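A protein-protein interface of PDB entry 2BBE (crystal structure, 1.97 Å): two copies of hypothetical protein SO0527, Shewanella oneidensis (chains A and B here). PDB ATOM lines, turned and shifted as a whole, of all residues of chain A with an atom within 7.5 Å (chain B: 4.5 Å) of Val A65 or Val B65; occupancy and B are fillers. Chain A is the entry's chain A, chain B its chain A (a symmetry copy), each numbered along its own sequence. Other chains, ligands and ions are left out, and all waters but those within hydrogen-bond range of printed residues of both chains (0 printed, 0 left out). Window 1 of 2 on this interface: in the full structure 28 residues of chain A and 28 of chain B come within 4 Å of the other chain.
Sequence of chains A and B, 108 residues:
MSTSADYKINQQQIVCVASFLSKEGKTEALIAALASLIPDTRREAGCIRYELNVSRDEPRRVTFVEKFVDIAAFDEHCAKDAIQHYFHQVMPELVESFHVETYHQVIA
Val A15 touches Asn B53 (CG2 to ND2, 3.5 Å). Val A65 touches Val B65. Asn B53 touches Tyr A103 (CB to CD2, 3.6 Å). Glu B51 touches Gln A105. CA of Gln A105 touches ND2 of Asn B53, 3.8 Å away.
Of the 10 printed residues of chain B, 5 touch a printed residue of chain A.
NH1 of Arg A49 is in salt-bridge range of OE1 of Glu B51, at 2.8 Å. The side-chain carboxylate (OE1) of Glu A51 lies within salt-bridge range of the guanidinium group (NH1) of Arg B49 (2.8 Å). OE1 of Glu B51 lies within salt-bridge range of NZ of Lys A67 (3.4 Å). OH of Tyr A103 is in hydrogen-bond range of OG1 of Thr B63 (2.8 Å). The guanidinium group (NH2) of Arg A49 lies close to the guanidinium group (NE) of Arg B49 (3.4 Å).
O of Val A15 is in hydrogen-bond range of N of Tyr A103 (2.8 Å). The backbone NH of Ile A48 lies within hydrogen-bond range of the backbone carbonyl oxygen of Lys A67 (2.8 Å). The side-chain carboxylate (OE2) of Glu A51 is in salt-bridge range of the guanidinium group (NE) of Arg A49, 3.9 Å away. The side-chain amide oxygen of Asn A53 lies close to the backbone carbonyl oxygen of Glu A51 (3.1 Å). OE1 of Gln A105 is in hydrogen-bond range of NZ of Lys A67, at 3.1 Å. The backbone carbonyl oxygen (O) of Glu B51 lies within hydrogen-bond range of the backbone NH (N) of Val B65.
Of the printed residues of chain B, Val A15 touches Asn B53 (3.5 Å). Printed residues of chain B within 4 Å of Glu A51: Arg B49. Val A65 touches just one residue of chain B: Val B65. Glu A66 touches none of the printed residues of chain B. Printed residues of chain A within 4 Å of Val B65: Val A65 (3.7 Å). The nearest residue of chain A that does not touch Val B65 is Val A17 (4.3 Å). The nearest printed residue of chain A that does not touch Thr B63 is Val A17 (5.3 Å).
Arg B49 touches its own counterpart, Arg A49. Arg A49 touches Glu B51, and with the chains exchanged Glu A51 touches Arg B49. Val B65 touches its own counterpart, Val A65. Positions printed for both chains: 16, 17, 49, 50, 51, 53, 63, 64, 65 and 66.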
ATOM      1  N   VAL A  15      21.931  11.635   1.617  1.00  0.00           N
ATOM      2  CA  VAL A  15      20.711  11.556   2.423  1.00  0.00           C
ATOM      3  C   VAL A  15      20.728  12.721   3.417  1.00  0.00           C
ATOM      4  O   VAL A  15      21.784  13.068   3.943  1.00  0.00           O
ATOM      5  CB  VAL A  15      20.600  10.173   3.137  1.00  0.00           C
ATOM      6  CG1 VAL A  15      19.521  10.191   4.281  1.00  0.00           C
ATOM      7  CG2 VAL A  15      20.259   9.072   2.094  1.00  0.00           C
ATOM      8  N   CYS A  16      19.580  13.340   3.650  1.00  0.00           N
ATOM      9  CA  CYS A  16      19.501  14.381   4.675  1.00  0.00           C
ATOM     10  C   CYS A  16      18.277  14.189   5.535  1.00  0.00           C
ATOM     11  O   CYS A  16      17.168  13.908   5.023  1.00  0.00           O
ATOM     12  CB  CYS A  16      19.485  15.796   4.050  1.00  0.00           C
ATOM     13  SG  CYS A  16      19.353  17.150   5.267  1.00  0.00           S
ATOM     14  N   VAL A  17      18.468  14.324   6.843  1.00  0.00           N
ATOM     15  CA  VAL A  17      17.350  14.357   7.778  1.00  0.00           C
ATOM     16  C   VAL A  17      17.386  15.716   8.480  1.00  0.00           C
ATOM     17  O   VAL A  17      18.393  16.074   9.099  1.00  0.00           O
ATOM     18  CB  VAL A  17      17.405  13.214   8.814  1.00  0.00           C
ATOM     19  CG1 VAL A  17      16.231  13.336   9.810  1.00  0.00           C
ATOM     20  CG2 VAL A  17      17.365  11.828   8.105  1.00  0.00           C
ATOM     21  N   ALA A  18      16.302  16.473   8.372  1.00  0.00           N
ATOM     22  CA  ALA A  18      16.257  17.838   8.927  1.00  0.00           C
ATOM     23  C   ALA A  18      14.998  17.949   9.786  1.00  0.00           C
ATOM     24  O   ALA A  18      13.870  17.894   9.261  1.00  0.00           O
ATOM     25  CB  ALA A  18      16.249  18.887   7.761  1.00  0.00           C
ATOM     26  N   SER A  19      15.184  18.074  11.103  1.00  0.00           N
ATOM     27  CA  SER A  19      14.066  18.096  12.038  1.00  0.00           C
ATOM     28  C   SER A  19      13.942  19.481  12.615  1.00  0.00           C
ATOM     29  O   SER A  19      14.958  20.146  12.888  1.00  0.00           O
ATOM     30  CB  SER A  19      14.236  17.075  13.177  1.00  0.00           C
ATOM     31  OG  SER A  19      15.419  17.322  13.935  1.00  0.00           O
ATOM     32  N   ILE A  48      15.817  13.015  -5.323  1.00  0.00           N
ATOM     33  CA  ILE A  48      15.291  11.626  -5.356  1.00  0.00           C
ATOM     34  C   ILE A  48      14.091  11.484  -4.433  1.00  0.00           C
ATOM     35  O   ILE A  48      13.080  10.872  -4.795  1.00  0.00           O
ATOM     36  CB  ILE A  48      16.381  10.579  -4.960  1.00  0.00           C
ATOM     37  CG1 ILE A  48      17.543  10.595  -5.964  1.00  0.00           C
ATOM     38  CG2 ILE A  48      15.792   9.147  -4.778  1.00  0.00           C
ATOM     39  CD1 ILE A  48      18.810   9.805  -5.461  1.00  0.00           C
ATOM     40  N   ARG A  49      14.196  12.100  -3.256  1.00  0.00           N
ATOM     41  CA  ARG A  49      13.218  11.967  -2.202  1.00  0.00           C
ATOM     42  C   ARG A  49      13.163  13.254  -1.406  1.00  0.00           C
ATOM     43  O   ARG A  49      14.201  13.870  -1.081  1.00  0.00           O
ATOM     44  CB  ARG A  49      13.578  10.780  -1.265  1.00  0.00           C
ATOM     45  CG  ARG A  49      12.698  10.636  -0.064  1.00  0.00           C
ATOM     46  CD  ARG A  49      13.171   9.493   0.881  1.00  0.00           C
ATOM     47  NE  ARG A  49      13.274   8.212   0.173  1.00  0.00           N
ATOM     48  CZ  ARG A  49      14.051   7.199   0.558  1.00  0.00           C
ATOM     49  NH1 ARG A  49      14.807   7.311   1.649  1.00  0.00           N
ATOM     50  NH2 ARG A  49      14.058   6.069  -0.132  1.00  0.00           N
ATOM     51  N   TYR A  50      11.945  13.662  -1.080  1.00  0.00           N
ATOM     52  CA  TYR A  50      11.744  14.842  -0.230  1.00  0.00           C
ATOM     53  C   TYR A  50      10.427  14.713   0.518  1.00  0.00           C
ATOM     54  O   TYR A  50       9.377  15.216   0.067  1.00  0.00           O
ATOM     55  CB  TYR A  50      11.768  16.090  -1.104  1.00  0.00           C
ATOM     56  CG  TYR A  50      11.988  17.388  -0.377  1.00  0.00           C
ATOM     57  CD1 TYR A  50      13.197  17.650   0.299  1.00  0.00           C
ATOM     58  CD2 TYR A  50      11.016  18.376  -0.420  1.00  0.00           C
ATOM     59  CE1 TYR A  50      13.419  18.879   0.942  1.00  0.00           C
ATOM     60  CE2 TYR A  50      11.225  19.620   0.205  1.00  0.00           C
ATOM     61  CZ  TYR A  50      12.423  19.849   0.881  1.00  0.00           C
ATOM     62  OH  TYR A  50      12.597  21.067   1.473  1.00  0.00           O
ATOM     63  N   GLU A  51      10.486  14.025   1.655  1.00  0.00           N
ATOM     64  CA  GLU A  51       9.289  13.598   2.361  1.00  0.00           C
ATOM     65  C   GLU A  51       9.184  14.314   3.696  1.00  0.00           C
ATOM     66  O   GLU A  51      10.153  14.359   4.462  1.00  0.00           O
ATOM     67  CB  GLU A  51       9.328  12.088   2.597  1.00  0.00           C
ATOM     68  CG  GLU A  51       9.290  11.290   1.295  1.00  0.00           C
ATOM     69  CD  GLU A  51       9.428   9.800   1.537  1.00  0.00           C
ATOM     70  OE1 GLU A  51       9.524   9.372   2.715  1.00  0.00           O
ATOM     71  OE2 GLU A  51       9.433   9.055   0.535  1.00  0.00           O
ATOM     72  N   LEU A  52       8.005  14.875   3.955  1.00  0.00           N
ATOM     73  CA  LEU A  52       7.718  15.576   5.208  1.00  0.00           C
ATOM     74  C   LEU A  52       6.958  14.661   6.185  1.00  0.00           C
ATOM     75  O   LEU A  52       6.142  13.832   5.769  1.00  0.00           O
ATOM     76  CB  LEU A  52       6.898  16.846   4.908  1.00  0.00           C
ATOM     77  CG  LEU A  52       6.703  17.860   6.049  1.00  0.00           C
ATOM     78  CD1 LEU A  52       8.067  18.367   6.613  1.00  0.00           C
ATOM     79  CD2 LEU A  52       5.831  19.027   5.547  1.00  0.00           C
ATOM     80  N   ASN A  53       7.234  14.816   7.478  1.00  0.00           N
ATOM     81  CA  ASN A  53       6.760  13.884   8.501  1.00  0.00           C
ATOM     82  C   ASN A  53       6.455  14.652   9.793  1.00  0.00           C
ATOM     83  O   ASN A  53       7.211  15.569  10.178  1.00  0.00           O
ATOM     84  CB  ASN A  53       7.838  12.822   8.791  1.00  0.00           C
ATOM     85  CG  ASN A  53       8.359  12.133   7.518  1.00  0.00           C
ATOM     86  OD1 ASN A  53       9.302  12.610   6.856  1.00  0.00           O
ATOM     87  ND2 ASN A  53       7.737  11.036   7.167  1.00  0.00           N
ATOM     88  N   THR A  63       9.673  16.884  10.451  1.00  0.00           N
ATOM     89  CA  THR A  63      10.980  16.427   9.950  1.00  0.00           C
ATOM     90  C   THR A  63      10.957  16.078   8.467  1.00  0.00           C
ATOM     91  O   THR A  63      10.067  15.347   8.016  1.00  0.00           O
ATOM     92  CB  THR A  63      11.446  15.182  10.761  1.00  0.00           C
ATOM     93  OG1 THR A  63      11.587  15.556  12.133  1.00  0.00           O
ATOM     94  CG2 THR A  63      12.779  14.578  10.230  1.00  0.00           C
ATOM     95  N   PHE A  64      11.935  16.591   7.714  1.00  0.00           N
ATOM     96  CA  PHE A  64      12.140  16.176   6.338  1.00  0.00           C
ATOM     97  C   PHE A  64      13.108  14.993   6.249  1.00  0.00           C
ATOM     98  O   PHE A  64      14.172  14.988   6.885  1.00  0.00           O
ATOM     99  CB  PHE A  64      12.715  17.340   5.477  1.00  0.00           C
ATOM    100  CG  PHE A  64      11.668  18.114   4.710  1.00  0.00           C
ATOM    101  CD1 PHE A  64      10.866  17.477   3.750  1.00  0.00           C
ATOM    102  CD2 PHE A  64      11.507  19.488   4.921  1.00  0.00           C
ATOM    103  CE1 PHE A  64       9.903  18.200   3.030  1.00  0.00           C
ATOM    104  CE2 PHE A  64      10.561  20.212   4.199  1.00  0.00           C
ATOM    105  CZ  PHE A  64       9.748  19.568   3.278  1.00  0.00           C
ATOM    106  N   VAL A  65      12.744  14.022   5.418  1.00  0.00           N
ATOM    107  CA  VAL A  65      13.609  12.903   5.069  1.00  0.00           C
ATOM    108  C   VAL A  65      13.879  13.026   3.574  1.00  0.00           C
ATOM    109  O   VAL A  65      12.942  12.997   2.752  1.00  0.00           O
ATOM    110  CB  VAL A  65      12.926  11.556   5.416  1.00  0.00           C
ATOM    111  CG1 VAL A  65      13.689  10.355   4.758  1.00  0.00           C
ATOM    112  CG2 VAL A  65      12.832  11.422   6.965  1.00  0.00           C
ATOM    113  N   GLU A  66      15.154  13.197   3.226  1.00  0.00           N
ATOM    114  CA  GLU A  66      15.522  13.642   1.886  1.00  0.00           C
ATOM    115  C   GLU A  66      16.602  12.752   1.286  1.00  0.00           C
ATOM    116  O   GLU A  66      17.381  12.131   2.031  1.00  0.00           O
ATOM    117  CB  GLU A  66      16.073  15.090   1.940  1.00  0.00           C
ATOM    118  CG  GLU A  66      15.291  16.068   2.841  1.00  0.00           C
ATOM    119  CD  GLU A  66      15.966  17.447   2.962  1.00  0.00           C
ATOM    120  OE1 GLU A  66      16.957  17.722   2.242  1.00  0.00           O
ATOM    121  OE2 GLU A  66      15.487  18.273   3.780  1.00  0.00           O
ATOM    122  N   LYS A  67      16.658  12.736  -0.047  1.00  0.00           N
ATOM    123  CA  LYS A  67      17.742  12.074  -0.792  1.00  0.00           C
ATOM    124  C   LYS A  67      17.967  12.790  -2.121  1.00  0.00           C
ATOM    125  O   LYS A  67      17.008  13.154  -2.821  1.00  0.00           O
ATOM    126  CB  LYS A  67      17.449  10.577  -1.014  1.00  0.00           C
ATOM    127  CG  LYS A  67      18.694   9.727  -1.333  1.00  0.00           C
ATOM    128  CD  LYS A  67      18.362   8.253  -1.696  1.00  0.00           C
ATOM    129  CE  LYS A  67      17.901   7.409  -0.498  1.00  0.00           C
ATOM    130  NZ  LYS A  67      17.654   5.932  -0.860  1.00  0.00           N
ATOM    131  N   PHE A  68      19.240  12.997  -2.457  1.00  0.00           N
ATOM    132  CA  PHE A  68      19.670  13.688  -3.677  1.00  0.00           C
ATOM    133  C   PHE A  68      20.726  12.858  -4.387  1.00  0.00           C
ATOM    134  O   PHE A  68      21.434  12.060  -3.757  1.00  0.00           O
ATOM    135  CB  PHE A  68      20.230  15.092  -3.354  1.00  0.00           C
ATOM    136  CG  PHE A  68      19.206  16.005  -2.761  1.00  0.00           C
ATOM    137  CD1 PHE A  68      18.977  16.007  -1.379  1.00  0.00           C
ATOM    138  CD2 PHE A  68      18.427  16.828  -3.589  1.00  0.00           C
ATOM    139  CE1 PHE A  68      17.986  16.834  -0.817  1.00  0.00           C
ATOM    140  CE2 PHE A  68      17.435  17.649  -3.050  1.00  0.00           C
ATOM    141  CZ  PHE A  68      17.213  17.652  -1.669  1.00  0.00           C
ATOM    142  N   TYR A 103      24.058  12.365   5.342  1.00  0.00           N
ATOM    143  CA  TYR A 103      24.493  10.991   5.448  1.00  0.00           C
ATOM    144  C   TYR A 103      24.843  10.423   4.067  1.00  0.00           C
ATOM    145  O   TYR A 103      24.391  10.958   3.041  1.00  0.00           O
ATOM    146  CB  TYR A 103      23.323  10.149   5.947  1.00  0.00           C
ATOM    147  CG  TYR A 103      22.841  10.405   7.355  1.00  0.00           C
ATOM    148  CD1 TYR A 103      21.847  11.369   7.624  1.00  0.00           C
ATOM    149  CD2 TYR A 103      23.318   9.625   8.414  1.00  0.00           C
ATOM    150  CE1 TYR A 103      21.360  11.558   8.941  1.00  0.00           C
ATOM    151  CE2 TYR A 103      22.854   9.817   9.728  1.00  0.00           C
ATOM    152  CZ  TYR A 103      21.876  10.777   9.978  1.00  0.00           C
ATOM    153  OH  TYR A 103      21.408  10.945  11.266  1.00  0.00           O
ATOM    154  N   GLN A 105      24.291   6.506   2.358  1.00  0.00           N
ATOM    155  CA  GLN A 105      23.526   5.302   2.598  1.00  0.00           C
ATOM    156  C   GLN A 105      24.447   4.101   2.635  1.00  0.00           C
ATOM    157  O   GLN A 105      25.417   4.035   1.876  1.00  0.00           O
ATOM    158  CB  GLN A 105      22.426   5.122   1.545  1.00  0.00           C
ATOM    159  CG  GLN A 105      21.410   4.012   1.913  1.00  0.00           C
ATOM    160  CD  GLN A 105      20.328   3.796   0.844  1.00  0.00           C
ATOM    161  OE1 GLN A 105      20.300   4.475  -0.185  1.00  0.00           O
ATOM    162  NE2 GLN A 105      19.459   2.840   1.083  1.00  0.00           N
ATOM    163  N   CYS B  16       9.786   5.762  10.778  1.00  0.00           N
ATOM    164  CA  CYS B  16      10.644   5.794  11.963  1.00  0.00           C
ATOM    165  C   CYS B  16      12.041   6.225  11.597  1.00  0.00           C
ATOM    166  O   CYS B  16      12.612   5.763  10.581  1.00  0.00           O
ATOM    167  CB  CYS B  16      10.688   4.419  12.671  1.00  0.00           C
ATOM    168  SG  CYS B  16      11.768   4.368  14.142  1.00  0.00           S
ATOM    169  N   VAL B  17      12.598   7.119  12.408  1.00  0.00           N
ATOM    170  CA  VAL B  17      14.005   7.483  12.293  1.00  0.00           C
ATOM    171  C   VAL B  17      14.681   7.105  13.613  1.00  0.00           C
ATOM    172  O   VAL B  17      14.269   7.566  14.682  1.00  0.00           O
ATOM    173  CB  VAL B  17      14.209   8.984  11.993  1.00  0.00           C
ATOM    174  CG1 VAL B  17      15.715   9.320  11.941  1.00  0.00           C
ATOM    175  CG2 VAL B  17      13.525   9.373  10.650  1.00  0.00           C
ATOM    176  N   ARG B  49      10.295   0.288   3.851  1.00  0.00           N
ATOM    177  CA  ARG B  49      11.607   0.882   3.745  1.00  0.00           C
ATOM    178  C   ARG B  49      12.388   0.595   5.010  1.00  0.00           C
ATOM    179  O   ARG B  49      11.863   0.686   6.141  1.00  0.00           O
ATOM    180  CB  ARG B  49      11.500   2.417   3.526  1.00  0.00           C
ATOM    181  CG  ARG B  49      12.805   3.147   3.532  1.00  0.00           C
ATOM    182  CD  ARG B  49      12.621   4.688   3.407  1.00  0.00           C
ATOM    183  NE  ARG B  49      11.848   5.046   2.212  1.00  0.00           N
ATOM    184  CZ  ARG B  49      11.157   6.178   2.074  1.00  0.00           C
ATOM    185  NH1 ARG B  49      11.133   7.073   3.059  1.00  0.00           N
ATOM    186  NH2 ARG B  49      10.509   6.426   0.946  1.00  0.00           N
ATOM    187  N   TYR B  50      13.655   0.254   4.823  1.00  0.00           N
ATOM    188  CA  TYR B  50      14.557   0.040   5.962  1.00  0.00           C
ATOM    189  C   TYR B  50      15.989   0.327   5.539  1.00  0.00           C
ATOM    190  O   TYR B  50      16.740  -0.588   5.142  1.00  0.00           O
ATOM    191  CB  TYR B  50      14.398  -1.394   6.453  1.00  0.00           C
ATOM    192  CG  TYR B  50      14.922  -1.668   7.836  1.00  0.00           C
ATOM    193  CD1 TYR B  50      14.350  -1.053   8.969  1.00  0.00           C
ATOM    194  CD2 TYR B  50      15.942  -2.589   8.017  1.00  0.00           C
ATOM    195  CE1 TYR B  50      14.811  -1.341  10.264  1.00  0.00           C
ATOM    196  CE2 TYR B  50      16.408  -2.904   9.308  1.00  0.00           C
ATOM    197  CZ  TYR B  50      15.837  -2.269  10.411  1.00  0.00           C
ATOM    198  OH  TYR B  50      16.309  -2.599  11.649  1.00  0.00           O
ATOM    199  N   GLU B  51      16.357   1.603   5.615  1.00  0.00           N
ATOM    200  CA  GLU B  51      17.593   2.085   5.021  1.00  0.00           C
ATOM    201  C   GLU B  51      18.552   2.543   6.107  1.00  0.00           C
ATOM    202  O   GLU B  51      18.168   3.304   7.002  1.00  0.00           O
ATOM    203  CB  GLU B  51      17.304   3.250   4.074  1.00  0.00           C
ATOM    204  CG  GLU B  51      16.460   2.832   2.873  1.00  0.00           C
ATOM    205  CD  GLU B  51      16.097   4.014   1.995  1.00  0.00           C
ATOM    206  OE1 GLU B  51      16.522   5.159   2.294  1.00  0.00           O
ATOM    207  OE2 GLU B  51      15.387   3.787   0.993  1.00  0.00           O
ATOM    208  N   ASN B  53      22.232   4.424   7.235  1.00  0.00           N
ATOM    209  CA  ASN B  53      22.916   5.645   6.806  1.00  0.00           C
ATOM    210  C   ASN B  53      24.028   5.988   7.804  1.00  0.00           C
ATOM    211  O   ASN B  53      23.839   5.853   9.032  1.00  0.00           O
ATOM    212  CB  ASN B  53      21.917   6.817   6.743  1.00  0.00           C
ATOM    213  CG  ASN B  53      20.658   6.490   5.922  1.00  0.00           C
ATOM    214  OD1 ASN B  53      19.664   5.943   6.440  1.00  0.00           O
ATOM    215  ND2 ASN B  53      20.709   6.799   4.652  1.00  0.00           N
ATOM    216  N   THR B  63      22.300   5.808  11.376  1.00  0.00           N
ATOM    217  CA  THR B  63      20.858   6.078  11.491  1.00  0.00           C
ATOM    218  C   THR B  63      20.019   5.241  10.531  1.00  0.00           C
ATOM    219  O   THR B  63      20.329   5.174   9.336  1.00  0.00           O
ATOM    220  CB  THR B  63      20.583   7.588  11.226  1.00  0.00           C
ATOM    221  OG1 THR B  63      21.273   8.358  12.212  1.00  0.00           O
ATOM    222  CG2 THR B  63      19.067   7.939  11.236  1.00  0.00           C
ATOM    223  N   PHE B  64      18.959   4.615  11.051  1.00  0.00           N
ATOM    224  CA  PHE B  64      17.974   3.956  10.212  1.00  0.00           C
ATOM    225  C   PHE B  64      16.838   4.909   9.828  1.00  0.00           C
ATOM    226  O   PHE B  64      16.297   5.633  10.675  1.00  0.00           O
ATOM    227  CB  PHE B  64      17.350   2.724  10.935  1.00  0.00           C
ATOM    228  CG  PHE B  64      18.003   1.408  10.585  1.00  0.00           C
ATOM    229  CD1 PHE B  64      18.000   0.938   9.261  1.00  0.00           C
ATOM    230  CD2 PHE B  64      18.590   0.620  11.582  1.00  0.00           C
ATOM    231  CE1 PHE B  64      18.596  -0.291   8.939  1.00  0.00           C
ATOM    232  CE2 PHE B  64      19.171  -0.606  11.267  1.00  0.00           C
ATOM    233  CZ  PHE B  64      19.196  -1.047   9.953  1.00  0.00           C
ATOM    234  N   VAL B  65      16.461   4.859   8.555  1.00  0.00           N
ATOM    235  CA  VAL B  65      15.291   5.558   8.040  1.00  0.00           C
ATOM    236  C   VAL B  65      14.327   4.479   7.563  1.00  0.00           C
ATOM    237  O   VAL B  65      14.659   3.676   6.670  1.00  0.00           O
ATOM    238  CB  VAL B  65      15.691   6.514   6.888  1.00  0.00           C
ATOM    239  CG1 VAL B  65      14.424   7.022   6.116  1.00  0.00           C
ATOM    240  CG2 VAL B  65      16.537   7.684   7.473  1.00  0.00           C
ATOM    241  N   GLU B  66      13.147   4.439   8.183  1.00  0.00           N
ATOM    242  CA  GLU B  66      12.264   3.285   8.060  1.00  0.00           C
ATOM    243  C   GLU B  66      10.846   3.710   7.702  1.00  0.00           C
ATOM    244  O   GLU B  66      10.440   4.844   8.014  1.00  0.00           O
ATOM    245  CB  GLU B  66      12.206   2.515   9.404  1.00  0.00           C
ATOM    246  CG  GLU B  66      13.558   2.323  10.122  1.00  0.00           C
ATOM    247  CD  GLU B  66      13.416   1.677  11.513  1.00  0.00           C
ATOM    248  OE1 GLU B  66      12.302   1.234  11.884  1.00  0.00           O
ATOM    249  OE2 GLU B  66      14.439   1.601  12.239  1.00  0.00           O
